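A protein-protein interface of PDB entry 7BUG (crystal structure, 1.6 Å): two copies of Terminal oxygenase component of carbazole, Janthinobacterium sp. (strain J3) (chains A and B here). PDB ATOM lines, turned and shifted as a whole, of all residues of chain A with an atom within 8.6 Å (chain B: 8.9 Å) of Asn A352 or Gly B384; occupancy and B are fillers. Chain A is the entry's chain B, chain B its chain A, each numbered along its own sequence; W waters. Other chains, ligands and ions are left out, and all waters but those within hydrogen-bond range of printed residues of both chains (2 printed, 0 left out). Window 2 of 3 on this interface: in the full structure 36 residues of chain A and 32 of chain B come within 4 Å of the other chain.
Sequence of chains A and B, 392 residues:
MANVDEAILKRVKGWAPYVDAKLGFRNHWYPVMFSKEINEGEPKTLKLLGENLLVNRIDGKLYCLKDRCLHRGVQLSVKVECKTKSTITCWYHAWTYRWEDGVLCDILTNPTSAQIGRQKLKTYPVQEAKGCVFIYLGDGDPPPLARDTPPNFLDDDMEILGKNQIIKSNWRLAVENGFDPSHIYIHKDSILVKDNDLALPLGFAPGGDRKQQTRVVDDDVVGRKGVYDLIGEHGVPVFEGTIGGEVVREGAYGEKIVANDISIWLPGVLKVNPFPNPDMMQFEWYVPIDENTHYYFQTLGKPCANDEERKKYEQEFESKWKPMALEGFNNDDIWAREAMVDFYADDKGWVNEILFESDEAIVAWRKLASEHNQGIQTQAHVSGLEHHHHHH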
ATOM      1  N   ILE A   8     -26.342  -7.657  -4.620  1.00  0.00           N
ATOM      2  CA  ILE A   8     -26.300  -8.451  -5.874  1.00  0.00           C
ATOM      3  C   ILE A   8     -26.311  -9.941  -5.501  1.00  0.00           C
ATOM      4  O   ILE A   8     -27.055 -10.732  -6.095  1.00  0.00           O
ATOM      5  CB  ILE A   8     -25.061  -8.047  -6.713  1.00  0.00           C
ATOM      6  CG1 ILE A   8     -25.285  -6.665  -7.340  1.00  0.00           C
ATOM      7  CG2 ILE A   8     -24.815  -9.114  -7.760  1.00  0.00           C
ATOM      8  CD1 ILE A   8     -24.063  -5.856  -7.560  1.00  0.00           C
ATOM      9  N   ARG A  11     -29.421 -11.770  -4.833  1.00  0.00           N
ATOM     10  CA  ARG A  11     -30.280 -11.896  -6.034  1.00  0.00           C
ATOM     11  C   ARG A  11     -29.812 -13.001  -6.976  1.00  0.00           C
ATOM     12  O   ARG A  11     -30.534 -13.247  -7.920  1.00  0.00           O
ATOM     13  CB  ARG A  11     -30.314 -10.548  -6.743  1.00  0.00           C
ATOM     14  CG  ARG A  11     -30.970  -9.463  -5.910  1.00  0.00           C
ATOM     15  CD  ARG A  11     -31.050  -8.151  -6.640  1.00  0.00           C
ATOM     16  NE  ARG A  11     -32.173  -7.386  -6.122  1.00  0.00           N
ATOM     17  CZ  ARG A  11     -32.170  -6.679  -4.988  1.00  0.00           C
ATOM     18  NH1 ARG A  11     -31.092  -6.619  -4.217  1.00  0.00           N
ATOM     19  NH2 ARG A  11     -33.265  -6.022  -4.630  1.00  0.00           N
ATOM     20  N   VAL A  12     -28.686 -13.692  -6.727  1.00  0.00           N
ATOM     21  CA  VAL A  12     -28.188 -14.785  -7.612  1.00  0.00           C
ATOM     22  C   VAL A  12     -28.052 -16.133  -6.866  1.00  0.00           C
ATOM     23  O   VAL A  12     -27.058 -16.895  -7.096  1.00  0.00           O
ATOM     24  CB  VAL A  12     -26.843 -14.386  -8.241  1.00  0.00           C
ATOM     25  CG1 VAL A  12     -26.992 -13.182  -9.147  1.00  0.00           C
ATOM     26  CG2 VAL A  12     -25.804 -14.067  -7.215  1.00  0.00           C
ATOM     27  N   PHE A 343     -21.070  -4.618 -19.222  1.00  0.00           N
ATOM     28  CA  PHE A 343     -22.343  -5.032 -18.549  1.00  0.00           C
ATOM     29  C   PHE A 343     -22.073  -5.727 -17.212  1.00  0.00           C
ATOM     30  O   PHE A 343     -22.962  -5.621 -16.310  1.00  0.00           O
ATOM     31  CB  PHE A 343     -23.085  -5.993 -19.467  1.00  0.00           C
ATOM     32  CG  PHE A 343     -24.500  -6.360 -19.090  1.00  0.00           C
ATOM     33  CD1 PHE A 343     -25.439  -5.349 -18.942  1.00  0.00           C
ATOM     34  CD2 PHE A 343     -24.903  -7.685 -19.037  1.00  0.00           C
ATOM     35  CE1 PHE A 343     -26.785  -5.649 -18.727  1.00  0.00           C
ATOM     36  CE2 PHE A 343     -26.249  -7.988 -18.855  1.00  0.00           C
ATOM     37  CZ  PHE A 343     -27.178  -6.963 -18.728  1.00  0.00           C
ATOM     38  N   TYR A 344     -20.930  -6.383 -17.061  1.00  0.00           N
ATOM     39  CA  TYR A 344     -20.585  -7.153 -15.842  1.00  0.00           C
ATOM     40  C   TYR A 344     -19.675  -6.336 -14.914  1.00  0.00           C
ATOM     41  O   TYR A 344     -19.522  -6.795 -13.756  1.00  0.00           O
ATOM     42  CB  TYR A 344     -20.072  -8.550 -16.217  1.00  0.00           C
ATOM     43  CG  TYR A 344     -21.159  -9.423 -16.783  1.00  0.00           C
ATOM     44  CD1 TYR A 344     -22.033 -10.121 -15.967  1.00  0.00           C
ATOM     45  CD2 TYR A 344     -21.391  -9.475 -18.140  1.00  0.00           C
ATOM     46  CE1 TYR A 344     -23.044 -10.885 -16.496  1.00  0.00           C
ATOM     47  CE2 TYR A 344     -22.395 -10.245 -18.699  1.00  0.00           C
ATOM     48  CZ  TYR A 344     -23.261 -10.917 -17.864  1.00  0.00           C
ATOM     49  OH  TYR A 344     -24.280 -11.647 -18.430  1.00  0.00           O
ATOM     50  N   ASP A 346     -19.852  -3.617 -13.140  1.00  0.00           N
ATOM     51  CA  ASP A 346     -20.439  -3.058 -11.904  1.00  0.00           C
ATOM     52  C   ASP A 346     -21.151  -4.187 -11.159  1.00  0.00           C
ATOM     53  O   ASP A 346     -21.952  -3.894 -10.234  1.00  0.00           O
ATOM     54  CB  ASP A 346     -21.374  -1.929 -12.311  1.00  0.00           C
ATOM     55  CG  ASP A 346     -22.505  -2.354 -13.253  1.00  0.00           C
ATOM     56  OD1 ASP A 346     -22.586  -3.552 -13.593  1.00  0.00           O
ATOM     57  OD2 ASP A 346     -23.262  -1.454 -13.712  1.00  0.00           O
ATOM     58  N   ASP A 347     -20.927  -5.426 -11.613  1.00  0.00           N
ATOM     59  CA  ASP A 347     -21.568  -6.651 -11.074  1.00  0.00           C
ATOM     60  C   ASP A 347     -23.061  -6.735 -11.378  1.00  0.00           C
ATOM     61  O   ASP A 347     -23.651  -7.749 -11.015  1.00  0.00           O
ATOM     62  CB  ASP A 347     -21.329  -6.758  -9.566  1.00  0.00           C
ATOM     63  CG  ASP A 347     -19.866  -6.892  -9.207  1.00  0.00           C
ATOM     64  OD1 ASP A 347     -19.128  -7.626  -9.903  1.00  0.00           O
ATOM     65  OD2 ASP A 347     -19.452  -6.235  -8.227  1.00  0.00           O
ATOM     66  N   LYS A 348     -23.662  -5.753 -12.047  1.00  0.00           N
ATOM     67  CA  LYS A 348     -25.131  -5.751 -12.249  1.00  0.00           C
ATOM     68  C   LYS A 348     -25.527  -6.708 -13.368  1.00  0.00           C
ATOM     69  O   LYS A 348     -26.663  -7.191 -13.364  1.00  0.00           O
ATOM     70  CB  LYS A 348     -25.620  -4.320 -12.471  1.00  0.00           C
ATOM     71  CG  LYS A 348     -25.564  -3.457 -11.211  1.00  0.00           C
ATOM     72  CD  LYS A 348     -25.836  -1.971 -11.478  1.00  0.00           C
ATOM     73  CE  LYS A 348     -25.417  -1.042 -10.350  1.00  0.00           C
ATOM     74  NZ  LYS A 348     -25.831   0.349 -10.653  1.00  0.00           N
ATOM     75  N   GLY A 349     -24.651  -6.982 -14.334  1.00  0.00           N
ATOM     76  CA  GLY A 349     -24.980  -7.922 -15.404  1.00  0.00           C
ATOM     77  C   GLY A 349     -25.459  -9.269 -14.907  1.00  0.00           C
ATOM     78  O   GLY A 349     -26.247  -9.919 -15.566  1.00  0.00           O
ATOM     79  N   TRP A 350     -24.945  -9.741 -13.774  1.00  0.00           N
ATOM     80  CA  TRP A 350     -25.283 -11.066 -13.233  1.00  0.00           C
ATOM     81  C   TRP A 350     -26.761 -11.050 -12.862  1.00  0.00           C
ATOM     82  O   TRP A 350     -27.355 -12.139 -12.899  1.00  0.00           O
ATOM     83  CB  TRP A 350     -24.417 -11.371 -12.019  1.00  0.00           C
ATOM     84  CG  TRP A 350     -22.945 -11.361 -12.311  1.00  0.00           C
ATOM     85  CD1 TRP A 350     -22.030 -10.460 -11.842  1.00  0.00           C
ATOM     86  CD2 TRP A 350     -22.212 -12.302 -13.108  1.00  0.00           C
ATOM     87  NE1 TRP A 350     -20.794 -10.773 -12.331  1.00  0.00           N
ATOM     88  CE2 TRP A 350     -20.859 -11.909 -13.077  1.00  0.00           C
ATOM     89  CE3 TRP A 350     -22.550 -13.435 -13.860  1.00  0.00           C
ATOM     90  CZ2 TRP A 350     -19.870 -12.623 -13.732  1.00  0.00           C
ATOM     91  CZ3 TRP A 350     -21.569 -14.140 -14.516  1.00  0.00           C
ATOM     92  CH2 TRP A 350     -20.236 -13.712 -14.484  1.00  0.00           C
ATOM     93  N   VAL A 351     -27.326  -9.879 -12.526  1.00  0.00           N
ATOM     94  CA  VAL A 351     -28.770  -9.743 -12.188  1.00  0.00           C
ATOM     95  C   VAL A 351     -29.584  -9.418 -13.436  1.00  0.00           C
ATOM     96  O   VAL A 351     -30.678  -9.895 -13.556  1.00  0.00           O
ATOM     97  CB  VAL A 351     -29.020  -8.674 -11.119  1.00  0.00           C
ATOM     98  CG1 VAL A 351     -30.505  -8.618 -10.787  1.00  0.00           C
ATOM     99  CG2 VAL A 351     -28.184  -8.926  -9.883  1.00  0.00           C
ATOM    100  N   ASN A 352     -29.033  -8.624 -14.336  1.00  0.00           N
ATOM    101  CA  ASN A 352     -29.853  -7.974 -15.385  1.00  0.00           C
ATOM    102  C   ASN A 352     -29.829  -8.735 -16.720  1.00  0.00           C
ATOM    103  O   ASN A 352     -30.685  -8.453 -17.590  1.00  0.00           O
ATOM    104  CB  ASN A 352     -29.336  -6.573 -15.600  1.00  0.00           C
ATOM    105  CG  ASN A 352     -29.747  -5.635 -14.479  1.00  0.00           C
ATOM    106  OD1 ASN A 352     -29.173  -4.552 -14.379  1.00  0.00           O
ATOM    107  ND2 ASN A 352     -30.786  -6.022 -13.747  1.00  0.00           N
ATOM    108  N   GLU A 353     -28.910  -9.678 -16.877  1.00  0.00           N
ATOM    109  CA  GLU A 353     -28.884 -10.548 -18.072  1.00  0.00           C
ATOM    110  C   GLU A 353     -30.229 -11.265 -18.249  1.00  0.00           C
ATOM    111  O   GLU A 353     -30.936 -11.578 -17.226  1.00  0.00           O
ATOM    112  CB  GLU A 353     -27.750 -11.558 -17.973  1.00  0.00           C
ATOM    113  CG  GLU A 353     -27.923 -12.580 -16.884  1.00  0.00           C
ATOM    114  CD  GLU A 353     -26.812 -13.558 -16.578  1.00  0.00           C
ATOM    115  OE1 GLU A 353     -25.646 -13.364 -17.034  1.00  0.00           O
ATOM    116  OE2 GLU A 353     -27.133 -14.568 -15.833  1.00  0.00           O
ATOM    117  N   ILE A 354     -30.610 -11.505 -19.476  1.00  0.00           N
ATOM    118  CA  ILE A 354     -31.776 -12.364 -19.787  1.00  0.00           C
ATOM    119  C   ILE A 354     -31.287 -13.570 -20.562  1.00  0.00           C
ATOM    120  O   ILE A 354     -30.908 -13.470 -21.759  1.00  0.00           O
ATOM    121  CB  ILE A 354     -32.845 -11.572 -20.536  1.00  0.00           C
ATOM    122  CG1 ILE A 354     -33.262 -10.316 -19.753  1.00  0.00           C
ATOM    123  CG2 ILE A 354     -33.997 -12.543 -20.861  1.00  0.00           C
ATOM    124  CD1 ILE A 354     -34.201  -9.434 -20.497  1.00  0.00           C
ATOM    125  N   LEU A 355     -31.263 -14.705 -19.907  1.00  0.00           N
ATOM    126  CA  LEU A 355     -30.735 -15.936 -20.508  1.00  0.00           C
ATOM    127  C   LEU A 355     -31.795 -16.612 -21.369  1.00  0.00           C
ATOM    128  O   LEU A 355     -32.980 -16.366 -21.176  1.00  0.00           O
ATOM    129  CB  LEU A 355     -30.282 -16.866 -19.390  1.00  0.00           C
ATOM    130  CG  LEU A 355     -29.155 -16.292 -18.521  1.00  0.00           C
ATOM    131  CD1 LEU A 355     -28.617 -17.356 -17.585  1.00  0.00           C
ATOM    132  CD2 LEU A 355     -28.014 -15.691 -19.341  1.00  0.00           C
ATOM    133  N   LYS B  66     -31.862   1.144 -27.906  1.00  0.00           N
ATOM    134  CA  LYS B  66     -30.751   1.092 -26.928  1.00  0.00           C
ATOM    135  C   LYS B  66     -29.670   0.175 -27.495  1.00  0.00           C
ATOM    136  O   LYS B  66     -29.944  -0.945 -27.873  1.00  0.00           O
ATOM    137  CB  LYS B  66     -31.241   0.702 -25.545  1.00  0.00           C
ATOM    138  CG  LYS B  66     -30.093   0.557 -24.550  1.00  0.00           C
ATOM    139  CD  LYS B  66     -30.662   0.532 -23.141  1.00  0.00           C
ATOM    140  CE  LYS B  66     -31.178   1.871 -22.692  1.00  0.00           C
ATOM    141  NZ  LYS B  66     -31.324   1.937 -21.233  1.00  0.00           N
ATOM    142  N   ARG B  68     -27.612  -2.023 -26.394  1.00  0.00           N
ATOM    143  CA  ARG B  68     -27.283  -2.938 -25.263  1.00  0.00           C
ATOM    144  C   ARG B  68     -28.188  -4.145 -25.444  1.00  0.00           C
ATOM    145  O   ARG B  68     -29.418  -4.022 -25.198  1.00  0.00           O
ATOM    146  CB  ARG B  68     -27.460  -2.316 -23.893  1.00  0.00           C
ATOM    147  CG  ARG B  68     -26.950  -3.235 -22.789  1.00  0.00           C
ATOM    148  CD  ARG B  68     -26.988  -2.669 -21.380  1.00  0.00           C
ATOM    149  NE  ARG B  68     -28.374  -2.446 -21.096  1.00  0.00           N
ATOM    150  CZ  ARG B  68     -28.861  -1.560 -20.230  1.00  0.00           C
ATOM    151  NH1 ARG B  68     -28.058  -0.851 -19.464  1.00  0.00           N
ATOM    152  NH2 ARG B  68     -30.151  -1.394 -20.138  1.00  0.00           N
ATOM    153  N   CYS B  69     -27.643  -5.256 -25.929  1.00  0.00           N
ATOM    154  CA  CYS B  69     -28.422  -6.489 -26.123  1.00  0.00           C
ATOM    155  C   CYS B  69     -29.095  -6.912 -24.797  1.00  0.00           C
ATOM    156  O   CYS B  69     -28.455  -6.867 -23.745  1.00  0.00           O
ATOM    157  CB  CYS B  69     -27.552  -7.586 -26.700  1.00  0.00           C
ATOM    158  SG  CYS B  69     -28.527  -9.024 -27.198  1.00  0.00           S
ATOM    159  N   LEU B  70     -30.335  -7.384 -24.864  1.00  0.00           N
ATOM    160  CA  LEU B  70     -31.067  -7.918 -23.678  1.00  0.00           C
ATOM    161  C   LEU B  70     -30.397  -9.157 -23.098  1.00  0.00           C
ATOM    162  O   LEU B  70     -30.613  -9.477 -21.930  1.00  0.00           O
ATOM    163  CB  LEU B  70     -32.484  -8.279 -24.103  1.00  0.00           C
ATOM    164  CG  LEU B  70     -33.374  -7.123 -24.487  1.00  0.00           C
ATOM    165  CD1 LEU B  70     -34.779  -7.634 -24.836  1.00  0.00           C
ATOM    166  CD2 LEU B  70     -33.417  -6.020 -23.455  1.00  0.00           C
ATOM    167  N   HIS B  71     -29.666  -9.913 -23.903  1.00  0.00           N
ATOM    168  CA  HIS B  71     -29.153 -11.243 -23.524  1.00  0.00           C
ATOM    169  C   HIS B  71     -27.936 -11.085 -22.581  1.00  0.00           C
ATOM    170  O   HIS B  71     -28.060 -11.296 -21.367  1.00  0.00           O
ATOM    171  CB  HIS B  71     -28.871 -12.015 -24.825  1.00  0.00           C
ATOM    172  CG  HIS B  71     -28.313 -13.350 -24.604  1.00  0.00           C
ATOM    173  ND1 HIS B  71     -27.354 -13.859 -25.459  1.00  0.00           N
ATOM    174  CD2 HIS B  71     -28.559 -14.269 -23.648  1.00  0.00           C
ATOM    175  CE1 HIS B  71     -27.034 -15.079 -25.055  1.00  0.00           C
ATOM    176  NE2 HIS B  71     -27.806 -15.364 -23.917  1.00  0.00           N
ATOM    177  N   ARG B  72     -26.769 -10.744 -23.138  1.00  0.00           N
ATOM    178  CA  ARG B  72     -25.511 -10.623 -22.345  1.00  0.00           C
ATOM    179  C   ARG B  72     -25.029  -9.173 -22.296  1.00  0.00           C
ATOM    180  O   ARG B  72     -23.891  -8.919 -21.850  1.00  0.00           O
ATOM    181  CB  ARG B  72     -24.436 -11.591 -22.855  1.00  0.00           C
ATOM    182  CG  ARG B  72     -24.877 -13.050 -22.894  1.00  0.00           C
ATOM    183  CD  ARG B  72     -25.340 -13.684 -21.594  1.00  0.00           C
ATOM    184  NE  ARG B  72     -24.321 -13.545 -20.557  1.00  0.00           N
ATOM    185  CZ  ARG B  72     -23.283 -14.338 -20.375  1.00  0.00           C
ATOM    186  NH1 ARG B  72     -23.151 -15.429 -21.100  1.00  0.00           N
ATOM    187  NH2 ARG B  72     -22.435 -14.053 -19.414  1.00  0.00           N
ATOM    188  N   GLY B  73     -25.818  -8.208 -22.737  1.00  0.00           N
ATOM    189  CA  GLY B  73     -25.542  -6.780 -22.519  1.00  0.00           C
ATOM    190  C   GLY B  73     -24.400  -6.211 -23.319  1.00  0.00           C
ATOM    191  O   GLY B  73     -23.846  -5.183 -22.928  1.00  0.00           O
ATOM    192  N   TRP B  95     -29.799 -12.691 -31.409  1.00  0.00           N
ATOM    193  CA  TRP B  95     -31.091 -12.090 -31.023  1.00  0.00           C
ATOM    194  C   TRP B  95     -31.383 -10.938 -31.969  1.00  0.00           C
ATOM    195  O   TRP B  95     -30.569 -10.044 -32.202  1.00  0.00           O
ATOM    196  CB  TRP B  95     -31.119 -11.628 -29.569  1.00  0.00           C
ATOM    197  CG  TRP B  95     -31.066 -12.718 -28.564  1.00  0.00           C
ATOM    198  CD1 TRP B  95     -30.433 -13.925 -28.630  1.00  0.00           C
ATOM    199  CD2 TRP B  95     -31.668 -12.640 -27.270  1.00  0.00           C
ATOM    200  NE1 TRP B  95     -30.630 -14.623 -27.465  1.00  0.00           N
ATOM    201  CE2 TRP B  95     -31.361 -13.849 -26.612  1.00  0.00           C
ATOM    202  CE3 TRP B  95     -32.384 -11.644 -26.605  1.00  0.00           C
ATOM    203  CZ2 TRP B  95     -31.763 -14.078 -25.294  1.00  0.00           C
ATOM    204  CZ3 TRP B  95     -32.821 -11.905 -25.314  1.00  0.00           C
ATOM    205  CH2 TRP B  95     -32.508 -13.109 -24.687  1.00  0.00           C
ATOM    206  N   GLN B 119     -39.978 -10.381 -25.327  1.00  0.00           N
ATOM    207  CA  GLN B 119     -38.997  -9.386 -24.832  1.00  0.00           C
ATOM    208  C   GLN B 119     -38.980  -8.214 -25.823  1.00  0.00           C
ATOM    209  O   GLN B 119     -39.298  -8.357 -27.037  1.00  0.00           O
ATOM    210  CB  GLN B 119     -37.586  -9.970 -24.704  1.00  0.00           C
ATOM    211  CG  GLN B 119     -37.451 -11.162 -23.769  1.00  0.00           C
ATOM    212  CD  GLN B 119     -37.656 -10.896 -22.302  1.00  0.00           C
ATOM    213  OE1 GLN B 119     -37.767  -9.746 -21.849  1.00  0.00           O
ATOM    214  NE2 GLN B 119     -37.713 -11.968 -21.538  1.00  0.00           N
ATOM    215  N   THR B 378     -30.743   9.042 -13.588  1.00  0.00           N
ATOM    216  CA  THR B 378     -29.896   8.413 -12.548  1.00  0.00           C
ATOM    217  C   THR B 378     -29.195   7.176 -13.105  1.00  0.00           C
ATOM    218  O   THR B 378     -29.487   6.749 -14.214  1.00  0.00           O
ATOM    219  CB  THR B 378     -30.733   7.986 -11.329  1.00  0.00           C
ATOM    220  OG1 THR B 378     -31.453   6.815 -11.706  1.00  0.00           O
ATOM    221  CG2 THR B 378     -31.678   9.064 -10.855  1.00  0.00           C
ATOM    222  N   GLN B 379     -28.205   6.721 -12.362  1.00  0.00           N
ATOM    223  CA  GLN B 379     -27.405   5.542 -12.755  1.00  0.00           C
ATOM    224  C   GLN B 379     -28.371   4.359 -12.826  1.00  0.00           C
ATOM    225  O   GLN B 379     -28.131   3.438 -13.636  1.00  0.00           O
ATOM    226  CB  GLN B 379     -26.202   5.350 -11.817  1.00  0.00           C
ATOM    227  CG  GLN B 379     -24.883   5.876 -12.363  1.00  0.00           C
ATOM    228  CD  GLN B 379     -24.509   5.409 -13.748  1.00  0.00           C
ATOM    229  OE1 GLN B 379     -24.590   4.223 -14.113  1.00  0.00           O
ATOM    230  NE2 GLN B 379     -24.055   6.357 -14.540  1.00  0.00           N
ATOM    231  N   ALA B 380     -29.475   4.367 -12.079  1.00  0.00           N
ATOM    232  CA  ALA B 380     -30.498   3.314 -12.169  1.00  0.00           C
ATOM    233  C   ALA B 380     -31.114   3.292 -13.578  1.00  0.00           C
ATOM    234  O   ALA B 380     -31.363   2.217 -14.081  1.00  0.00           O
ATOM    235  CB  ALA B 380     -31.571   3.479 -11.099  1.00  0.00           C
ATOM    236  N   HIS B 381     -31.375   4.447 -14.209  1.00  0.00           N
ATOM    237  CA  HIS B 381     -31.897   4.458 -15.578  1.00  0.00           C
ATOM    238  C   HIS B 381     -30.826   3.875 -16.502  1.00  0.00           C
ATOM    239  O   HIS B 381     -31.164   3.149 -17.459  1.00  0.00           O
ATOM    240  CB  HIS B 381     -32.244   5.874 -16.012  1.00  0.00           C
ATOM    241  CG  HIS B 381     -33.372   6.491 -15.243  1.00  0.00           C
ATOM    242  ND1 HIS B 381     -33.179   7.446 -14.229  1.00  0.00           N
ATOM    243  CD2 HIS B 381     -34.711   6.325 -15.374  1.00  0.00           C
ATOM    244  CE1 HIS B 381     -34.367   7.808 -13.772  1.00  0.00           C
ATOM    245  NE2 HIS B 381     -35.334   7.145 -14.478  1.00  0.00           N
ATOM    246  N   VAL B 382     -29.578   4.212 -16.264  1.00  0.00           N
ATOM    247  CA  VAL B 382     -28.461   3.810 -17.155  1.00  0.00           C
ATOM    248  C   VAL B 382     -28.289   2.295 -17.081  1.00  0.00           C
ATOM    249  O   VAL B 382     -28.126   1.655 -18.149  1.00  0.00           O
ATOM    250  CB  VAL B 382     -27.162   4.530 -16.813  1.00  0.00           C
ATOM    251  CG1 VAL B 382     -26.044   4.037 -17.696  1.00  0.00           C
ATOM    252  CG2 VAL B 382     -27.316   6.040 -16.945  1.00  0.00           C
ATOM    253  N   SER B 383     -28.226   1.756 -15.871  1.00  0.00           N
ATOM    254  CA  SER B 383     -28.069   0.288 -15.667  1.00  0.00           C
ATOM    255  C   SER B 383     -29.397  -0.297 -15.181  1.00  0.00           C
ATOM    256  O   SER B 383     -30.146  -0.861 -16.020  1.00  0.00           O
ATOM    257  CB  SER B 383     -26.946   0.012 -14.732  1.00  0.00           C
ATOM    258  OG  SER B 383     -25.836   0.817 -15.085  1.00  0.00           O
ATOM    259  N   GLY B 384     -29.712  -0.114 -13.896  1.00  0.00           N
ATOM    260  CA  GLY B 384     -30.889  -0.746 -13.260  1.00  0.00           C
ATOM    261  C   GLY B 384     -30.602  -2.187 -12.885  1.00  0.00           C
ATOM    262  O   GLY B 384     -29.928  -2.394 -11.868  1.00  0.00           O
HETATM  263  O   HOH W   1     -30.922  -7.497 -20.115  1.00  0.00           O
HETATM  264  O   HOH W   2     -20.988  -5.017 -22.108  1.00  0.00           O
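Arg B68 touches Phe A343. Phe A343 touches Arg B72 (CD2 to O, 3.2 Å). CG of Phe A343 touches CA of Gly B73 (3.6 Å). Ser B383 touches Asp A346. CB of Ser B383 touches CD of Lys A348, 3.97 Å away. His B71 touches Glu A353 (O to CB, 3.4 Å). O of Ile A354 touches CH2 of Trp B95 (3.4 Å). CG2 of Ile A354 touches NE2 of Gln B119 (3.8 Å).
Asn A352 touches one residue of chain B. Of the printed residues of chain B, Glu A353 touches His B71 (3.4 Å) and Arg B72 (3.8 Å). Of the printed residues of chain A, Gln B119 touches Ile A354 (3.8 Å). Of chain A, only Asp A346 (3.7 Å) and Lys A348 (3.97 Å) come within 4 Å of Ser B383. The nearest residue of chain A that does not touch Gly B384 is Lys A348 (4.1 Å). The nearest printed residue of chain B that does not touch Tyr A344 is His B71 (4.8 Å).
The side-chain carboxylate (OE1) of Glu A353 lies within salt-bridge range of the guanidinium group (NE) of Arg B72, at 3.8 Å. NE of Arg B72 sits at hydrogen-bond distance from OH of Tyr A344 (2.9 Å). The backbone carbonyl oxygen (O) of His B71 is in hydrogen-bond range of the backbone NH (N) of Ile A354, 3.2 Å away. The backbone carbonyl oxygen (O) of Leu B70 lies within hydrogen-bond range of the backbone NH (N) of Ile A354 (3.2 Å). The side-chain amide oxygen of Asn A352 sits close to the backbone carbonyl oxygen of Gly B384, 3.4 Å away.
Water W1 bridges O of Leu B70 (2.7 Å) and O of Asn A352 (2.7 Å). Water W2 lies within hydrogen-bond range of the backbone NH (N) of Phe A343 (2.9 Å) and the backbone carbonyl oxygen (O) of Gly B73 (3.0 Å).
The side-chain hydroxyl (OH) of Tyr A344 lies within hydrogen-bond range of the side-chain carboxylate (OE1) of Glu A353, at 2.6 Å. O of Phe A343 lies within hydrogen-bond range of N of Gly A349, 2.9 Å away. SG of Cys B69 sits close to N of His B71. The backbone carbonyl oxygen (O) of Val B382 is in hydrogen-bond range of the guanidinium group (NH1) of Arg B68, 2.8 Å away. N of Lys A348 lies within hydrogen-bond range of OD1 of Asp A346 (2.9 Å).
Of the 16 printed residues of chain B, 9 touch a printed residue of chain A. Hydrophobic or aromatic side chains of chain B that line the printed part of chain A: His B71 and Trp B95. Of the 15 printed residues of chain A, 7 touch a printed residue of chain B. Printed residues of chain A that touch a printed residue of chain B: Phe A343, Tyr A344, Asp A346, Lys A348, Asn A352, Glu A353 and Ile A354.
No position is printed for both chains. Of the 13 pairs that touch across the chains among the printed residues, none has its exchanged pair printed and touching as well.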
